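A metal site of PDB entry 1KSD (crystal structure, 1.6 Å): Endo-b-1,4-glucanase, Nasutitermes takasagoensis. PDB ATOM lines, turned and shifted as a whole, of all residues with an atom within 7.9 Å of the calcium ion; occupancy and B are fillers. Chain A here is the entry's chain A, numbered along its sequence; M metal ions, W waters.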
ATOM      1  N   PHE A  63      39.354  19.590   2.414  1.00  0.00           N
ATOM      2  CA  PHE A  63      38.017  20.015   2.013  1.00  0.00           C
ATOM      3  C   PHE A  63      38.011  20.512   0.567  1.00  0.00           C
ATOM      4  O   PHE A  63      37.278  19.985  -0.269  1.00  0.00           O
ATOM      5  CB  PHE A  63      37.480  21.058   3.004  1.00  0.00           C
ATOM      6  CG  PHE A  63      36.004  21.338   2.879  1.00  0.00           C
ATOM      7  CD1 PHE A  63      35.110  20.333   2.472  1.00  0.00           C
ATOM      8  CD2 PHE A  63      35.487  22.587   3.194  1.00  0.00           C
ATOM      9  CE1 PHE A  63      33.739  20.590   2.384  1.00  0.00           C
ATOM     10  CE2 PHE A  63      34.115  22.852   3.112  1.00  0.00           C
ATOM     11  CZ  PHE A  63      33.240  21.854   2.713  1.00  0.00           C
ATOM     12  N   ASP A 150      31.085  17.639   6.620  1.00  0.00           N
ATOM     13  CA  ASP A 150      31.373  18.348   5.382  1.00  0.00           C
ATOM     14  C   ASP A 150      32.568  17.732   4.662  1.00  0.00           C
ATOM     15  O   ASP A 150      32.490  17.404   3.476  1.00  0.00           O
ATOM     16  CB  ASP A 150      31.626  19.834   5.657  1.00  0.00           C
ATOM     17  CG  ASP A 150      32.212  20.085   7.040  1.00  0.00           C
ATOM     18  OD1 ASP A 150      32.986  19.242   7.545  1.00  0.00           O
ATOM     19  OD2 ASP A 150      31.906  21.150   7.627  1.00  0.00           O
ATOM     20  N   GLU A 154      32.084  15.454   1.433  1.00  0.00           N
ATOM     21  CA  GLU A 154      32.631  15.852   0.134  1.00  0.00           C
ATOM     22  C   GLU A 154      33.574  14.791  -0.392  1.00  0.00           C
ATOM     23  O   GLU A 154      33.610  14.520  -1.591  1.00  0.00           O
ATOM     24  CB  GLU A 154      33.361  17.187   0.253  1.00  0.00           C
ATOM     25  CG  GLU A 154      33.770  17.772  -1.095  1.00  0.00           C
ATOM     26  CD  GLU A 154      32.578  18.030  -1.993  1.00  0.00           C
ATOM     27  OE1 GLU A 154      31.628  18.688  -1.527  1.00  0.00           O
ATOM     28  OE2 GLU A 154      32.583  17.572  -3.156  1.00  0.00           O
ATOM     29  N   ALA A 207      37.319  27.457   6.317  1.00  0.00           N
ATOM     30  CA  ALA A 207      36.281  27.202   7.307  1.00  0.00           C
ATOM     31  C   ALA A 207      35.001  26.778   6.603  1.00  0.00           C
ATOM     32  O   ALA A 207      34.644  27.309   5.563  1.00  0.00           O
ATOM     33  CB  ALA A 207      36.033  28.458   8.140  1.00  0.00           C
ATOM     34  N   SER A 208      34.309  25.806   7.183  1.00  0.00           N
ATOM     35  CA  SER A 208      33.052  25.344   6.608  1.00  0.00           C
ATOM     36  C   SER A 208      31.911  26.201   7.130  1.00  0.00           C
ATOM     37  O   SER A 208      31.834  26.460   8.326  1.00  0.00           O
ATOM     38  CB  SER A 208      32.803  23.890   6.974  1.00  0.00           C
ATOM     39  OG  SER A 208      31.509  23.493   6.552  1.00  0.00           O
ATOM     40  N   ALA A 209      31.050  26.663   6.231  1.00  0.00           N
ATOM     41  CA  ALA A 209      29.910  27.490   6.649  1.00  0.00           C
ATOM     42  C   ALA A 209      28.784  26.620   7.182  1.00  0.00           C
ATOM     43  O   ALA A 209      28.123  26.971   8.156  1.00  0.00           O
ATOM     44  CB  ALA A 209      29.409  28.320   5.469  1.00  0.00           C
ATOM     45  N   ASP A 210      28.569  25.475   6.541  1.00  0.00           N
ATOM     46  CA  ASP A 210      27.510  24.552   6.922  1.00  0.00           C
ATOM     47  C   ASP A 210      27.830  23.198   6.294  1.00  0.00           C
ATOM     48  O   ASP A 210      28.309  23.132   5.162  1.00  0.00           O
ATOM     49  CB  ASP A 210      26.175  25.092   6.380  1.00  0.00           C
ATOM     50  CG  ASP A 210      24.975  24.537   7.123  1.00  0.00           C
ATOM     51  OD1 ASP A 210      24.042  25.326   7.398  1.00  0.00           O
ATOM     52  OD2 ASP A 210      24.934  23.322   7.418  1.00  0.00           O
ATOM     53  N   TYR A 211      27.598  22.120   7.039  1.00  0.00           N
ATOM     54  CA  TYR A 211      27.883  20.779   6.534  1.00  0.00           C
ATOM     55  C   TYR A 211      26.666  20.074   5.973  1.00  0.00           C
ATOM     56  O   TYR A 211      26.778  19.041   5.331  1.00  0.00           O
ATOM     57  CB  TYR A 211      28.501  19.916   7.653  1.00  0.00           C
ATOM     58  CG  TYR A 211      27.570  19.674   8.840  1.00  0.00           C
ATOM     59  CD1 TYR A 211      26.474  18.828   8.730  1.00  0.00           C
ATOM     60  CD2 TYR A 211      27.806  20.304  10.064  1.00  0.00           C
ATOM     61  CE1 TYR A 211      25.617  18.609   9.816  1.00  0.00           C
ATOM     62  CE2 TYR A 211      26.960  20.091  11.144  1.00  0.00           C
ATOM     63  CZ  TYR A 211      25.876  19.257  11.020  1.00  0.00           C
ATOM     64  OH  TYR A 211      25.031  19.058  12.098  1.00  0.00           O
ATOM     65  N   ARG A 212      25.480  20.643   6.198  1.00  0.00           N
ATOM     66  CA  ARG A 212      24.254  20.018   5.728  1.00  0.00           C
ATOM     67  C   ARG A 212      24.160  19.823   4.219  1.00  0.00           C
ATOM     68  O   ARG A 212      23.644  18.795   3.759  1.00  0.00           O
ATOM     69  CB  ARG A 212      23.049  20.815   6.256  1.00  0.00           C
ATOM     70  CG  ARG A 212      22.972  20.792   7.781  1.00  0.00           C
ATOM     71  CD  ARG A 212      21.923  21.746   8.319  1.00  0.00           C
ATOM     72  NE  ARG A 212      21.843  21.696   9.782  1.00  0.00           N
ATOM     73  CZ  ARG A 212      22.835  22.051  10.594  1.00  0.00           C
ATOM     74  NH1 ARG A 212      23.989  22.483  10.108  1.00  0.00           N
ATOM     75  NH2 ARG A 212      22.670  21.970  11.913  1.00  0.00           N
ATOM     76  N   ASP A 213      24.664  20.770   3.433  1.00  0.00           N
ATOM     77  CA  ASP A 213      24.594  20.630   1.986  1.00  0.00           C
ATOM     78  C   ASP A 213      25.490  19.488   1.491  1.00  0.00           C
ATOM     79  O   ASP A 213      25.161  18.809   0.525  1.00  0.00           O
ATOM     80  CB  ASP A 213      24.942  21.947   1.273  1.00  0.00           C
ATOM     81  CG  ASP A 213      26.236  22.564   1.759  1.00  0.00           C
ATOM     82  OD1 ASP A 213      26.384  22.743   2.990  1.00  0.00           O
ATOM     83  OD2 ASP A 213      27.106  22.891   0.921  1.00  0.00           O
ATOM     84  N   GLU A 214      26.620  19.270   2.162  1.00  0.00           N
ATOM     85  CA  GLU A 214      27.515  18.173   1.770  1.00  0.00           C
ATOM     86  C   GLU A 214      26.874  16.816   1.987  1.00  0.00           C
ATOM     87  O   GLU A 214      27.133  15.866   1.239  1.00  0.00           O
ATOM     88  CB  GLU A 214      28.833  18.225   2.551  1.00  0.00           C
ATOM     89  CG  GLU A 214      29.869  19.223   2.045  1.00  0.00           C
ATOM     90  CD  GLU A 214      29.527  20.658   2.384  1.00  0.00           C
ATOM     91  OE1 GLU A 214      28.818  20.885   3.379  1.00  0.00           O
ATOM     92  OE2 GLU A 214      29.991  21.563   1.662  1.00  0.00           O
ATOM     93  N   LEU A 215      26.038  16.697   3.015  1.00  0.00           N
ATOM     94  CA  LEU A 215      25.383  15.425   3.286  1.00  0.00           C
ATOM     95  C   LEU A 215      24.432  15.071   2.142  1.00  0.00           C
ATOM     96  O   LEU A 215      24.373  13.924   1.706  1.00  0.00           O
ATOM     97  CB  LEU A 215      24.628  15.479   4.615  1.00  0.00           C
ATOM     98  CG  LEU A 215      25.503  15.527   5.874  1.00  0.00           C
ATOM     99  CD1 LEU A 215      24.614  15.721   7.101  1.00  0.00           C
ATOM    100  CD2 LEU A 215      26.308  14.234   5.998  1.00  0.00           C
ATOM    101  N   TRP A 247      18.118  27.888   0.076  1.00  0.00           N
ATOM    102  CA  TRP A 247      19.488  28.298   0.377  1.00  0.00           C
ATOM    103  C   TRP A 247      20.030  29.183  -0.742  1.00  0.00           C
ATOM    104  O   TRP A 247      19.592  29.061  -1.891  1.00  0.00           O
ATOM    105  CB  TRP A 247      20.393  27.073   0.521  1.00  0.00           C
ATOM    106  CG  TRP A 247      20.227  26.328   1.814  1.00  0.00           C
ATOM    107  CD1 TRP A 247      19.058  26.085   2.479  1.00  0.00           C
ATOM    108  CD2 TRP A 247      21.262  25.672   2.553  1.00  0.00           C
ATOM    109  NE1 TRP A 247      19.307  25.317   3.594  1.00  0.00           N
ATOM    110  CE2 TRP A 247      20.649  25.046   3.666  1.00  0.00           C
ATOM    111  CE3 TRP A 247      22.648  25.555   2.394  1.00  0.00           C
ATOM    112  CZ2 TRP A 247      21.374  24.310   4.606  1.00  0.00           C
ATOM    113  CZ3 TRP A 247      23.363  24.820   3.332  1.00  0.00           C
ATOM    114  CH2 TRP A 247      22.724  24.213   4.418  1.00  0.00           C
ATOM    115  N   ASN A 252      30.676  26.069  -5.039  1.00  0.00           N
ATOM    116  CA  ASN A 252      32.083  26.333  -4.762  1.00  0.00           C
ATOM    117  C   ASN A 252      32.510  25.339  -3.689  1.00  0.00           C
ATOM    118  O   ASN A 252      31.689  24.540  -3.235  1.00  0.00           O
ATOM    119  CB  ASN A 252      32.293  27.787  -4.310  1.00  0.00           C
ATOM    120  CG  ASN A 252      31.390  28.166  -3.167  1.00  0.00           C
ATOM    121  OD1 ASN A 252      31.488  27.617  -2.077  1.00  0.00           O
ATOM    122  ND2 ASN A 252      30.488  29.117  -3.420  1.00  0.00           N
ATOM    123  N   TRP A 253      33.771  25.375  -3.271  1.00  0.00           N
ATOM    124  CA  TRP A 253      34.259  24.414  -2.280  1.00  0.00           C
ATOM    125  C   TRP A 253      33.492  24.411  -0.961  1.00  0.00           C
ATOM    126  O   TRP A 253      33.489  23.412  -0.246  1.00  0.00           O
ATOM    127  CB  TRP A 253      35.744  24.647  -1.990  1.00  0.00           C
ATOM    128  CG  TRP A 253      36.050  25.970  -1.371  1.00  0.00           C
ATOM    129  CD1 TRP A 253      36.451  27.107  -2.002  1.00  0.00           C
ATOM    130  CD2 TRP A 253      35.941  26.306   0.028  1.00  0.00           C
ATOM    131  NE1 TRP A 253      36.590  28.138  -1.100  1.00  0.00           N
ATOM    132  CE2 TRP A 253      36.288  27.674   0.155  1.00  0.00           C
ATOM    133  CE3 TRP A 253      35.593  25.592   1.175  1.00  0.00           C
ATOM    134  CZ2 TRP A 253      36.281  28.331   1.391  1.00  0.00           C
ATOM    135  CZ3 TRP A 253      35.587  26.241   2.404  1.00  0.00           C
ATOM    136  CH2 TRP A 253      35.937  27.606   2.503  1.00  0.00           C
ATOM    137  N   ASP A 254      32.838  25.518  -0.641  1.00  0.00           N
ATOM    138  CA  ASP A 254      32.106  25.664   0.610  1.00  0.00           C
ATOM    139  C   ASP A 254      30.625  25.312   0.497  1.00  0.00           C
ATOM    140  O   ASP A 254      30.069  24.647   1.378  1.00  0.00           O
ATOM    141  CB  ASP A 254      32.252  27.109   1.084  1.00  0.00           C
ATOM    142  CG  ASP A 254      31.851  27.314   2.525  1.00  0.00           C
ATOM    143  OD1 ASP A 254      31.635  28.477   2.906  1.00  0.00           O
ATOM    144  OD2 ASP A 254      31.771  26.323   3.288  1.00  0.00           O
ATOM    145  N   SER A 255      29.997  25.745  -0.587  1.00  0.00           N
ATOM    146  CA  SER A 255      28.573  25.495  -0.803  1.00  0.00           C
ATOM    147  C   SER A 255      28.295  24.613  -2.007  1.00  0.00           C
ATOM    148  O   SER A 255      28.735  24.906  -3.122  1.00  0.00           O
ATOM    149  CB  SER A 255      27.845  26.837  -0.966  1.00  0.00           C
ATOM    150  OG  SER A 255      26.462  26.621  -1.174  1.00  0.00           O
ATOM    151  N   LYS A 256      27.525  23.553  -1.800  1.00  0.00           N
ATOM    152  CA  LYS A 256      27.200  22.629  -2.877  1.00  0.00           C
ATOM    153  C   LYS A 256      25.763  22.794  -3.365  1.00  0.00           C
ATOM    154  O   LYS A 256      25.334  22.083  -4.268  1.00  0.00           O
ATOM    155  CB  LYS A 256      27.410  21.185  -2.393  1.00  0.00           C
ATOM    156  CG  LYS A 256      28.710  20.988  -1.625  1.00  0.00           C
ATOM    157  CD  LYS A 256      29.916  21.223  -2.514  1.00  0.00           C
ATOM    158  CE  LYS A 256      31.043  21.942  -1.786  1.00  0.00           C
ATOM    159  NZ  LYS A 256      31.525  21.191  -0.595  1.00  0.00           N
ATOM    160  N   VAL A 257      25.052  23.750  -2.786  1.00  0.00           N
ATOM    161  CA  VAL A 257      23.650  24.000  -3.121  1.00  0.00           C
ATOM    162  C   VAL A 257      23.241  23.867  -4.588  1.00  0.00           C
ATOM    163  O   VAL A 257      22.405  23.022  -4.932  1.00  0.00           O
ATOM    164  CB  VAL A 257      23.196  25.392  -2.613  1.00  0.00           C
ATOM    165  CG1 VAL A 257      21.773  25.693  -3.091  1.00  0.00           C
ATOM    166  CG2 VAL A 257      23.263  25.432  -1.092  1.00  0.00           C
HETATM  167 CA    CA M   1      28.751  23.342   2.854  1.00  0.00          CA
HETATM  168  O   HOH W   1      30.845  23.958   3.972  1.00  0.00           O
HETATM  169  O   HOH W   2      27.997  25.650   3.120  1.00  0.00           O
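OD2 of Asp 210 lies within salt-bridge range of NH1 of Arg 212. The backbone NH (N) of Lys 256 sits close to the side-chain carboxylate (OD2) of Asp 213. The side-chain amide oxygen of Asn 252 lies within hydrogen-bond range of the backbone NH of Asp 254 (2.9 Å). OE2 of Glu 214 sits close to NZ of Lys 256 (2.8 Å). OD2 of Asp 254 lies within hydrogen-bond range of N of Ala 209 (3.0 Å).
Within 4 Å of the calcium ion: Asp 210, Asp 213, Glu 214 and Asp 254. Along chain A the residues within 4 Å of the calcium ion span positions 210 to 254.
The calcium ion is bound by the backbone carbonyl oxygen (O) of Asp 210 (2.4 Å), the backbone carbonyl oxygen (O) of Asp 254 (2.4 Å), water W2 (2.4 Å), the side-chain carboxylate (OD1) of Asp 213 (2.4 Å), water W1 (2.5 Å), the side-chain carboxylate (OE2) of Glu 214 (2.5 Å), the side-chain carboxylate (OE1) of Glu 214 (2.5 Å) and the side-chain carboxylate (OD2) of Asp 213 (2.6 Å).
Water W1 bridges OD2 of Asp 254 and OG of Ser 208.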
